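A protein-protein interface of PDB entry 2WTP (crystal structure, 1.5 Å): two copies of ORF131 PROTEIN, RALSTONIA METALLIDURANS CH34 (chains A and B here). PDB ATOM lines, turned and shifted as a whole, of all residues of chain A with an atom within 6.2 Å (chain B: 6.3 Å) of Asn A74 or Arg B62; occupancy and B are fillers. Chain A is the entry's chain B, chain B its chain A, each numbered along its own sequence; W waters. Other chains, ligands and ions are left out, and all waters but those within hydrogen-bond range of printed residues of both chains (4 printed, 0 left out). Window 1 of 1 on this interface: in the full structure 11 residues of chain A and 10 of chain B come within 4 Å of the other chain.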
ATOM      1  N   ARG A  62      20.178 -22.006  19.156  1.00  0.00           N
ATOM      2  CA  ARG A  62      20.457 -21.055  20.227  1.00  0.00           C
ATOM      3  C   ARG A  62      19.174 -20.580  20.820  1.00  0.00           C
ATOM      4  O   ARG A  62      18.073 -20.687  20.160  1.00  0.00           O
ATOM      5  CB  ARG A  62      21.238 -19.797  19.679  1.00  0.00           C
ATOM      6  CG  ARG A  62      20.528 -19.086  18.485  1.00  0.00           C
ATOM      7  CD  ARG A  62      21.217 -17.738  18.208  1.00  0.00           C
ATOM      8  NE  ARG A  62      20.723 -17.297  16.878  1.00  0.00           N
ATOM      9  CZ  ARG A  62      20.809 -16.009  16.494  1.00  0.00           C
ATOM     10  NH1 ARG A  62      21.296 -15.074  17.298  1.00  0.00           N
ATOM     11  NH2 ARG A  62      20.386 -15.737  15.235  1.00  0.00           N
ATOM     12  N   ILE A  64      17.610 -17.100  22.379  1.00  0.00           N
ATOM     13  CA  ILE A  64      17.746 -15.630  22.482  1.00  0.00           C
ATOM     14  C   ILE A  64      16.807 -15.172  23.581  1.00  0.00           C
ATOM     15  O   ILE A  64      15.594 -15.418  23.505  1.00  0.00           O
ATOM     16  CB  ILE A  64      17.374 -15.016  21.165  1.00  0.00           C
ATOM     17  CG1 ILE A  64      18.400 -15.402  20.079  1.00  0.00           C
ATOM     18  CG2 ILE A  64      17.449 -13.466  21.300  1.00  0.00           C
ATOM     19  CD1 ILE A  64      18.100 -14.797  18.691  1.00  0.00           C
ATOM     20  N   MET A  70      15.677  -4.329  22.892  1.00  0.00           N
ATOM     21  CA  MET A  70      16.738  -5.011  22.091  1.00  0.00           C
ATOM     22  C   MET A  70      16.817  -4.645  20.561  1.00  0.00           C
ATOM     23  O   MET A  70      17.890  -4.876  19.915  1.00  0.00           O
ATOM     24  CB  MET A  70      16.640  -6.518  22.273  1.00  0.00           C
ATOM     25  CG  MET A  70      15.451  -7.084  21.595  1.00  0.00           C
ATOM     26  SD  MET A  70      15.362  -8.860  22.020  1.00  0.00           S
ATOM     27  CE  MET A  70      16.869  -9.583  21.568  1.00  0.00           C
ATOM     28  N   ARG A  71      15.683  -4.096  20.041  1.00  0.00           N
ATOM     29  CA  ARG A  71      15.491  -3.592  18.700  1.00  0.00           C
ATOM     30  C   ARG A  71      15.332  -4.661  17.653  1.00  0.00           C
ATOM     31  O   ARG A  71      14.261  -4.710  16.935  1.00  0.00           O
ATOM     32  CB  ARG A  71      16.566  -2.592  18.250  1.00  0.00           C
ATOM     33  CG  ARG A  71      16.578  -1.328  19.120  1.00  0.00           C
ATOM     34  CD  ARG A  71      17.621  -0.327  18.531  1.00  0.00           C
ATOM     35  NE  ARG A  71      17.692   0.890  19.367  1.00  0.00           N
ATOM     36  CZ  ARG A  71      16.967   2.012  19.213  1.00  0.00           C
ATOM     37  NH1 ARG A  71      16.012   2.167  18.259  1.00  0.00           N
ATOM     38  NH2 ARG A  71      17.190   2.998  20.081  1.00  0.00           N
ATOM     39  N   TYR A  72      16.317  -5.560  17.471  1.00  0.00           N
ATOM     40  CA  TYR A  72      16.190  -6.574  16.433  1.00  0.00           C
ATOM     41  C   TYR A  72      17.163  -7.697  16.688  1.00  0.00           C
ATOM     42  O   TYR A  72      18.092  -7.521  17.482  1.00  0.00           O
ATOM     43  CB  TYR A  72      16.446  -5.943  15.060  1.00  0.00           C
ATOM     44  CG  TYR A  72      17.910  -5.456  14.754  1.00  0.00           C
ATOM     45  CD1 TYR A  72      18.869  -6.281  14.225  1.00  0.00           C
ATOM     46  CD2 TYR A  72      18.243  -4.166  15.083  1.00  0.00           C
ATOM     47  CE1 TYR A  72      20.152  -5.771  13.939  1.00  0.00           C
ATOM     48  CE2 TYR A  72      19.551  -3.658  14.848  1.00  0.00           C
ATOM     49  CZ  TYR A  72      20.445  -4.470  14.249  1.00  0.00           C
ATOM     50  OH  TYR A  72      21.732  -3.953  13.991  1.00  0.00           O
ATOM     51  N   VAL A  73      16.920  -8.772  15.964  1.00  0.00           N
ATOM     52  CA  VAL A  73      17.856  -9.906  15.834  1.00  0.00           C
ATOM     53  C   VAL A  73      18.013 -10.232  14.390  1.00  0.00           C
ATOM     54  O   VAL A  73      17.167  -9.872  13.561  1.00  0.00           O
ATOM     55  CB  VAL A  73      17.406 -11.143  16.637  1.00  0.00           C
ATOM     56  CG1 VAL A  73      17.177 -10.847  18.100  1.00  0.00           C
ATOM     57  CG2 VAL A  73      16.100 -11.661  16.068  1.00  0.00           C
ATOM     58  N   ASN A  74      19.070 -10.951  14.067  1.00  0.00           N
ATOM     59  CA  ASN A  74      19.341 -11.430  12.750  1.00  0.00           C
ATOM     60  C   ASN A  74      19.283 -12.915  12.700  1.00  0.00           C
ATOM     61  O   ASN A  74      20.007 -13.576  13.496  1.00  0.00           O
ATOM     62  CB  ASN A  74      20.759 -10.993  12.226  1.00  0.00           C
ATOM     63  CG  ASN A  74      20.854  -9.550  11.916  1.00  0.00           C
ATOM     64  OD1 ASN A  74      19.884  -8.763  11.910  1.00  0.00           O
ATOM     65  ND2 ASN A  74      22.079  -9.101  11.761  1.00  0.00           N
ATOM     66  N   VAL A  75      18.522 -13.503  11.782  1.00  0.00           N
ATOM     67  CA  VAL A  75      18.444 -14.970  11.643  1.00  0.00           C
ATOM     68  C   VAL A  75      18.667 -15.386  10.213  1.00  0.00           C
ATOM     69  O   VAL A  75      18.414 -14.541   9.300  1.00  0.00           O
ATOM     70  CB  VAL A  75      17.111 -15.533  12.186  1.00  0.00           C
ATOM     71  CG1 VAL A  75      16.886 -15.130  13.590  1.00  0.00           C
ATOM     72  CG2 VAL A  75      15.920 -15.091  11.297  1.00  0.00           C
ATOM     73  N   ASP A  76      19.114 -16.625  10.003  1.00  0.00           N
ATOM     74  CA  ASP A  76      19.294 -17.081   8.637  1.00  0.00           C
ATOM     75  C   ASP A  76      18.066 -17.844   8.183  1.00  0.00           C
ATOM     76  O   ASP A  76      17.350 -18.444   8.958  1.00  0.00           O
ATOM     77  CB  ASP A  76      20.534 -17.984   8.606  1.00  0.00           C
ATOM     78  CG  ASP A  76      21.347 -17.834   7.342  1.00  0.00           C
ATOM     79  OD1 ASP A  76      20.753 -17.375   6.311  1.00  0.00           O
ATOM     80  OD2 ASP A  76      22.532 -18.198   7.434  1.00  0.00           O
ATOM     81  N   GLU A  79      17.376 -21.358   9.801  1.00  0.00           N
ATOM     82  CA  GLU A  79      17.824 -21.465  11.198  1.00  0.00           C
ATOM     83  C   GLU A  79      16.667 -21.740  12.109  1.00  0.00           C
ATOM     84  O   GLU A  79      15.553 -21.197  11.906  1.00  0.00           O
ATOM     85  CB  GLU A  79      18.508 -20.106  11.563  1.00  0.00           C
ATOM     86  CG  GLU A  79      19.339 -20.101  12.889  1.00  0.00           C
ATOM     87  CD  GLU A  79      19.907 -18.753  13.242  1.00  0.00           C
ATOM     88  OE1 GLU A  79      19.840 -17.817  12.442  1.00  0.00           O
ATOM     89  OE2 GLU A  79      20.504 -18.657  14.343  1.00  0.00           O
ATOM     90  N   ARG A 119      12.184  -6.555  15.831  1.00  0.00           N
ATOM     91  CA  ARG A 119      12.264  -6.906  14.444  1.00  0.00           C
ATOM     92  C   ARG A 119      13.167  -8.083  14.234  1.00  0.00           C
ATOM     93  O   ARG A 119      14.261  -8.160  14.831  1.00  0.00           O
ATOM     94  CB  ARG A 119      12.773  -5.694  13.664  1.00  0.00           C
ATOM     95  CG  ARG A 119      12.783  -5.838  12.210  1.00  0.00           C
ATOM     96  CD  ARG A 119      12.506  -4.496  11.542  1.00  0.00           C
ATOM     97  NE  ARG A 119      11.374  -4.759  10.649  1.00  0.00           N
ATOM     98  CZ  ARG A 119      10.138  -5.037  11.066  1.00  0.00           C
ATOM     99  NH1 ARG A 119       9.203  -5.339  10.179  1.00  0.00           N
ATOM    100  NH2 ARG A 119       9.849  -5.028  12.374  1.00  0.00           N
ATOM    101  N   VAL A 120      12.769  -9.010  13.353  1.00  0.00           N
ATOM    102  CA  VAL A 120      13.594 -10.152  12.976  1.00  0.00           C
ATOM    103  C   VAL A 120      14.015  -9.944  11.533  1.00  0.00           C
ATOM    104  O   VAL A 120      13.175  -9.907  10.653  1.00  0.00           O
ATOM    105  CB  VAL A 120      12.783 -11.505  13.106  1.00  0.00           C
ATOM    106  CG1 VAL A 120      13.701 -12.657  12.733  1.00  0.00           C
ATOM    107  CG2 VAL A 120      12.277 -11.614  14.535  1.00  0.00           C
ATOM    108  N   TYR A 121      15.296  -9.768  11.264  1.00  0.00           N
ATOM    109  CA  TYR A 121      15.791  -9.665   9.900  1.00  0.00           C
ATOM    110  C   TYR A 121      16.172 -11.039   9.419  1.00  0.00           C
ATOM    111  O   TYR A 121      17.025 -11.701  10.055  1.00  0.00           O
ATOM    112  CB  TYR A 121      17.028  -8.707   9.880  1.00  0.00           C
ATOM    113  CG  TYR A 121      16.693  -7.266  10.041  1.00  0.00           C
ATOM    114  CD1 TYR A 121      16.297  -6.529   8.936  1.00  0.00           C
ATOM    115  CD2 TYR A 121      16.742  -6.682  11.261  1.00  0.00           C
ATOM    116  CE1 TYR A 121      15.926  -5.207   9.100  1.00  0.00           C
ATOM    117  CE2 TYR A 121      16.414  -5.348  11.498  1.00  0.00           C
ATOM    118  CZ  TYR A 121      15.992  -4.643  10.366  1.00  0.00           C
ATOM    119  OH  TYR A 121      15.642  -3.312  10.534  1.00  0.00           O
ATOM    120  N   ILE A 122      15.555 -11.562   8.387  1.00  0.00           N
ATOM    121  CA  ILE A 122      15.842 -12.924   7.958  1.00  0.00           C
ATOM    122  C   ILE A 122      16.611 -12.837   6.670  1.00  0.00           C
ATOM    123  O   ILE A 122      16.253 -12.187   5.669  1.00  0.00           O
ATOM    124  CB  ILE A 122      14.512 -13.647   7.581  1.00  0.00           C
ATOM    125  CG1 ILE A 122      13.553 -13.597   8.795  1.00  0.00           C
ATOM    126  CG2 ILE A 122      14.866 -15.091   7.245  1.00  0.00           C
ATOM    127  CD1 ILE A 122      12.090 -14.002   8.349  1.00  0.00           C
ATOM    128  N   ALA B  60      26.243   2.496  16.937  1.00  0.00           N
ATOM    129  CA  ALA B  60      25.722   1.125  16.845  1.00  0.00           C
ATOM    130  C   ALA B  60      24.221   1.125  16.674  1.00  0.00           C
ATOM    131  O   ALA B  60      23.498   1.915  17.278  1.00  0.00           O
ATOM    132  CB  ALA B  60      26.094   0.398  18.156  1.00  0.00           C
ATOM    133  N   SER B  61      23.743   0.119  15.926  1.00  0.00           N
ATOM    134  CA  SER B  61      22.313   0.013  15.647  1.00  0.00           C
ATOM    135  C   SER B  61      21.632  -0.908  16.660  1.00  0.00           C
ATOM    136  O   SER B  61      20.406  -0.965  16.702  1.00  0.00           O
ATOM    137  CB  SER B  61      22.016  -0.540  14.260  1.00  0.00           C
ATOM    138  OG  SER B  61      22.830  -1.609  13.934  1.00  0.00           O
ATOM    139  N   ARG B  62      22.375  -1.636  17.487  1.00  0.00           N
ATOM    140  CA  ARG B  62      21.798  -2.432  18.590  1.00  0.00           C
ATOM    141  C   ARG B  62      22.891  -2.730  19.633  1.00  0.00           C
ATOM    142  O   ARG B  62      24.075  -2.592  19.277  1.00  0.00           O
ATOM    143  CB  ARG B  62      21.170  -3.725  18.127  1.00  0.00           C
ATOM    144  CG  ARG B  62      22.183  -4.639  17.390  1.00  0.00           C
ATOM    145  CD  ARG B  62      21.581  -6.076  17.087  1.00  0.00           C
ATOM    146  NE  ARG B  62      22.410  -6.725  16.074  1.00  0.00           N
ATOM    147  CZ  ARG B  62      22.403  -8.024  15.883  1.00  0.00           C
ATOM    148  NH1 ARG B  62      21.765  -8.824  16.701  1.00  0.00           N
ATOM    149  NH2 ARG B  62      23.083  -8.489  14.847  1.00  0.00           N
ATOM    150  N   ILE B  63      22.488  -3.133  20.818  1.00  0.00           N
ATOM    151  CA  ILE B  63      23.466  -3.551  21.862  1.00  0.00           C
ATOM    152  C   ILE B  63      23.112  -4.995  22.158  1.00  0.00           C
ATOM    153  O   ILE B  63      21.913  -5.359  22.463  1.00  0.00           O
ATOM    154  CB  ILE B  63      23.252  -2.732  23.132  1.00  0.00           C
ATOM    155  CG1 ILE B  63      23.568  -1.306  22.867  1.00  0.00           C
ATOM    156  CG2 ILE B  63      24.196  -3.210  24.219  1.00  0.00           C
ATOM    157  CD1 ILE B  63      23.179  -0.349  24.033  1.00  0.00           C
ATOM    158  N   ILE B  64      24.119  -5.890  22.023  1.00  0.00           N
ATOM    159  CA  ILE B  64      23.891  -7.337  22.279  1.00  0.00           C
ATOM    160  C   ILE B  64      24.491  -7.593  23.679  1.00  0.00           C
ATOM    161  O   ILE B  64      25.655  -7.294  23.947  1.00  0.00           O
ATOM    162  CB  ILE B  64      24.655  -8.167  21.233  1.00  0.00           C
ATOM    163  CG1 ILE B  64      23.981  -7.999  19.865  1.00  0.00           C
ATOM    164  CG2 ILE B  64      24.559  -9.668  21.612  1.00  0.00           C
ATOM    165  CD1 ILE B  64      24.685  -8.742  18.761  1.00  0.00           C
ATOM    166  N   VAL B  73      26.207 -15.172  17.694  1.00  0.00           N
ATOM    167  CA  VAL B  73      25.257 -14.150  17.223  1.00  0.00           C
ATOM    168  C   VAL B  73      25.480 -13.977  15.751  1.00  0.00           C
ATOM    169  O   VAL B  73      26.519 -14.340  15.216  1.00  0.00           O
ATOM    170  CB  VAL B  73      25.452 -12.778  17.867  1.00  0.00           C
ATOM    171  CG1 VAL B  73      25.126 -12.844  19.359  1.00  0.00           C
ATOM    172  CG2 VAL B  73      26.854 -12.298  17.723  1.00  0.00           C
ATOM    173  N   ASN B  74      24.473 -13.486  15.017  1.00  0.00           N
ATOM    174  CA  ASN B  74      24.595 -13.188  13.582  1.00  0.00           C
ATOM    175  C   ASN B  74      24.663 -11.714  13.339  1.00  0.00           C
ATOM    176  O   ASN B  74      23.818 -10.996  13.856  1.00  0.00           O
ATOM    177  CB  ASN B  74      23.360 -13.731  12.818  1.00  0.00           C
ATOM    178  CG  ASN B  74      23.272 -15.205  12.740  1.00  0.00           C
ATOM    179  OD1 ASN B  74      24.206 -15.968  12.860  1.00  0.00           O
ATOM    180  ND2 ASN B  74      22.044 -15.684  12.541  1.00  0.00           N
ATOM    181  N   VAL B  75      25.645 -11.275  12.561  1.00  0.00           N
ATOM    182  CA  VAL B  75      25.722  -9.839  12.151  1.00  0.00           C
ATOM    183  C   VAL B  75      25.888  -9.795  10.671  1.00  0.00           C
ATOM    184  O   VAL B  75      26.265 -10.742   9.961  1.00  0.00           O
ATOM    185  CB  VAL B  75      26.916  -9.145  12.827  1.00  0.00           C
ATOM    186  CG1 VAL B  75      26.790  -9.288  14.387  1.00  0.00           C
ATOM    187  CG2 VAL B  75      28.307  -9.688  12.332  1.00  0.00           C
ATOM    188  N   ASP B  76      25.535  -8.632  10.129  1.00  0.00           N
ATOM    189  CA  ASP B  76      25.758  -8.384   8.723  1.00  0.00           C
ATOM    190  C   ASP B  76      27.142  -7.764   8.482  1.00  0.00           C
ATOM    191  O   ASP B  76      27.689  -7.034   9.295  1.00  0.00           O
ATOM    192  CB  ASP B  76      24.722  -7.363   8.221  1.00  0.00           C
ATOM    193  CG  ASP B  76      23.306  -7.928   8.160  1.00  0.00           C
ATOM    194  OD1 ASP B  76      23.136  -9.149   7.900  1.00  0.00           O
ATOM    195  OD2 ASP B  76      22.380  -7.124   8.474  1.00  0.00           O
ATOM    196  N   GLU B  79      27.737  -4.064   9.503  1.00  0.00           N
ATOM    197  CA  GLU B  79      26.900  -3.630  10.666  1.00  0.00           C
ATOM    198  C   GLU B  79      27.721  -3.103  11.803  1.00  0.00           C
ATOM    199  O   GLU B  79      28.864  -3.642  12.037  1.00  0.00           O
ATOM    200  CB  GLU B  79      26.134  -4.867  11.139  1.00  0.00           C
ATOM    201  CG  GLU B  79      24.929  -4.595  12.136  1.00  0.00           C
ATOM    202  CD  GLU B  79      24.182  -5.878  12.612  1.00  0.00           C
ATOM    203  OE1 GLU B  79      24.460  -6.948  12.138  1.00  0.00           O
ATOM    204  OE2 GLU B  79      23.349  -5.726  13.536  1.00  0.00           O
ATOM    205  N   THR B  80      27.254  -2.088  12.521  1.00  0.00           N
ATOM    206  CA  THR B  80      27.949  -1.581  13.690  1.00  0.00           C
ATOM    207  C   THR B  80      27.105  -2.011  14.891  1.00  0.00           C
ATOM    208  O   THR B  80      25.940  -1.676  15.025  1.00  0.00           O
ATOM    209  CB  THR B  80      28.106  -0.046  13.708  1.00  0.00           C
ATOM    210  OG1 THR B  80      28.877   0.327  12.556  1.00  0.00           O
ATOM    211  CG2 THR B  80      28.873   0.389  14.972  1.00  0.00           C
ATOM    212  N   VAL B  81      27.722  -2.815  15.756  1.00  0.00           N
ATOM    213  CA  VAL B  81      27.030  -3.506  16.884  1.00  0.00           C
ATOM    214  C   VAL B  81      27.779  -3.214  18.124  1.00  0.00           C
ATOM    215  O   VAL B  81      29.054  -3.276  18.138  1.00  0.00           O
ATOM    216  CB  VAL B  81      27.045  -5.058  16.642  1.00  0.00           C
ATOM    217  CG1 VAL B  81      26.336  -5.743  17.778  1.00  0.00           C
ATOM    218  CG2 VAL B  81      26.325  -5.403  15.312  1.00  0.00           C
ATOM    219  N   ALA B  82      27.058  -2.921  19.190  1.00  0.00           N
ATOM    220  CA  ALA B  82      27.706  -2.783  20.492  1.00  0.00           C
ATOM    221  C   ALA B  82      27.442  -4.008  21.318  1.00  0.00           C
ATOM    222  O   ALA B  82      26.381  -4.689  21.160  1.00  0.00           O
ATOM    223  CB  ALA B  82      27.132  -1.515  21.206  1.00  0.00           C
ATOM    224  N   PHE B  83      28.472  -4.421  22.057  1.00  0.00           N
ATOM    225  CA  PHE B  83      28.361  -5.604  22.893  1.00  0.00           C
ATOM    226  C   PHE B  83      28.524  -5.192  24.338  1.00  0.00           C
ATOM    227  O   PHE B  83      29.433  -4.403  24.662  1.00  0.00           O
ATOM    228  CB  PHE B  83      29.485  -6.569  22.521  1.00  0.00           C
ATOM    229  CG  PHE B  83      29.348  -7.162  21.115  1.00  0.00           C
ATOM    230  CD1 PHE B  83      28.631  -8.323  20.900  1.00  0.00           C
ATOM    231  CD2 PHE B  83      29.869  -6.464  19.999  1.00  0.00           C
ATOM    232  CE1 PHE B  83      28.537  -8.869  19.576  1.00  0.00           C
ATOM    233  CE2 PHE B  83      29.756  -6.960  18.716  1.00  0.00           C
ATOM    234  CZ  PHE B  83      29.062  -8.173  18.496  1.00  0.00           C
HETATM  235  O   HOH W   1      20.006  -6.679  10.100  1.00  0.00           O
HETATM  236  O   HOH W   2      23.211 -11.361   9.790  1.00  0.00           O
HETATM  237  O   HOH W   3      19.927  -6.483  20.989  1.00  0.00           O
HETATM  238  O   HOH W   4      20.045  -8.496  19.109  1.00  0.00           O
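The side-chain hydroxyl (OH) of Tyr A72 sits at hydrogen-bond distance from the side-chain hydroxyl (OG) of Ser B61 (2.6 Å). The guanidinium group (NH2) of Arg B62 sits close to the side-chain amide nitrogen (ND2) of Asn A74 (3.3 Å). The side-chain amide nitrogen of Asn B74 lies close to the guanidinium group of Arg A62 (3.2 Å). The backbone carbonyl oxygen of Asn A74 lies within hydrogen-bond range of the side-chain amide nitrogen of Asn B74, at 3.1 Å. ND2 of Asn B74 sits at hydrogen-bond distance from OE1 of Glu A79 (3.1 Å). The side-chain hydroxyl of Tyr A72 lies within hydrogen-bond range of the side-chain carboxylate of Glu B79 (2.4 Å). The side-chain amide nitrogen (ND2) of Asn A74 is in hydrogen-bond range of the side-chain carboxylate (OE1) of Glu B79, at 3.2 Å.
The backbone carbonyl oxygen of Thr B80 is in hydrogen-bond range of the backbone NH of Ser B61 (3.0 Å). The guanidinium group (NH2) of Arg B62 is in hydrogen-bond range of the backbone carbonyl oxygen (O) of Asn B74 (2.8 Å). The guanidinium group (NE) of Arg B62 lies within salt-bridge range of the side-chain carboxylate (OE2) of Glu B79 (2.9 Å). N of Ala B82 sits at hydrogen-bond distance from O of Arg B62 (3.0 Å). The guanidinium group (NE) of Arg A62 is in salt-bridge range of the side-chain carboxylate (OE2) of Glu A79 (2.9 Å). N of Asp A76 lies within hydrogen-bond range of OE1 of Glu A79, 2.8 Å away.
Among the printed residues, pairs that only touch across the chains: Met A70 with Arg B62 (3.9 Å), Arg A71 with Ser B61 (3.4 Å), Tyr A72 with Arg B62 (3.3 Å), Asn A74 with Val B75 (3.7 Å), Asn A74 with Asp B76 (3.8 Å), Val A75 with Asn B74 (3.8 Å) and Asp A76 with Asn B74 (3.99 Å).
Of the printed residues of chain B, Asn A74 touches Arg B62 (3.3 Å), Asn B74 (3.1 Å), Val B75 (3.7 Å), Asp B76 (3.8 Å) and Glu B79 (3.2 Å). Of chain A, only Met A70 (3.9 Å), Tyr A72 (3.3 Å) and Asn A74 (3.3 Å) come within 4 Å of Arg B62. Printed residues of chain B within 4 Å of Glu A79: Asn B74. Of the printed residues of chain A, Ser B61 touches Arg A71 and Tyr A72. Printed residues of chain B within 4 Å of Val A75: Asn B74 (3.8 Å). Of the printed residues of chain A, Asn B74 touches Arg A62 (3.2 Å), Asn A74 (3.1 Å), Val A75 (3.8 Å), Asp A76 (3.99 Å) and Glu A79 (3.1 Å). Printed residues of chain B within 4 Å of Arg A62: Asn B74. The nearest residue of chain A that does not touch Arg B62 is Val A73 (4.1 Å). The nearest printed residue of chain A that does not touch Glu B79 is Val A73 (7.0 Å).
Of the 14 printed residues of chain A, 8 touch a printed residue of chain B. Of the 14 printed residues of chain B, 6 touch a printed residue of chain A. Along chain B the printed residues that touch a printed residue of chain A span positions 61 to 79.
Arg A62 touches Asn B74, and with the chains exchanged Asn A74 touches Arg B62. Asn B74 touches its own counterpart, Asn A74. Asn A74 touches Asp B76, and with the chains exchanged Asp A76 touches Asn B74. Asn A74 touches Glu B79, and with the chains exchanged Glu A79 touches Asn B74. Of the 14 pairs that touch across the chains among the printed residues, 9 have their exchanged pair printed and touching as well.
Water W3 bridges the backbone carbonyl oxygen of Ile B63 and the backbone carbonyl oxygen of Met A70. Water W4 lies within hydrogen-bond range of the backbone carbonyl oxygen (O) of Tyr A72 and the guanidinium group (NH1) of Arg B62. Water W1 bridges OD1 of Asn A74 and OD2 of Asp B76. Water W2 lies within hydrogen-bond range of the side-chain carboxylate (OD1) of Asp B76 (2.9 Å), the backbone carbonyl oxygen (O) of Val B75 (3.1 Å) and the side-chain amide nitrogen (ND2) of Asn A74 (3.2 Å).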
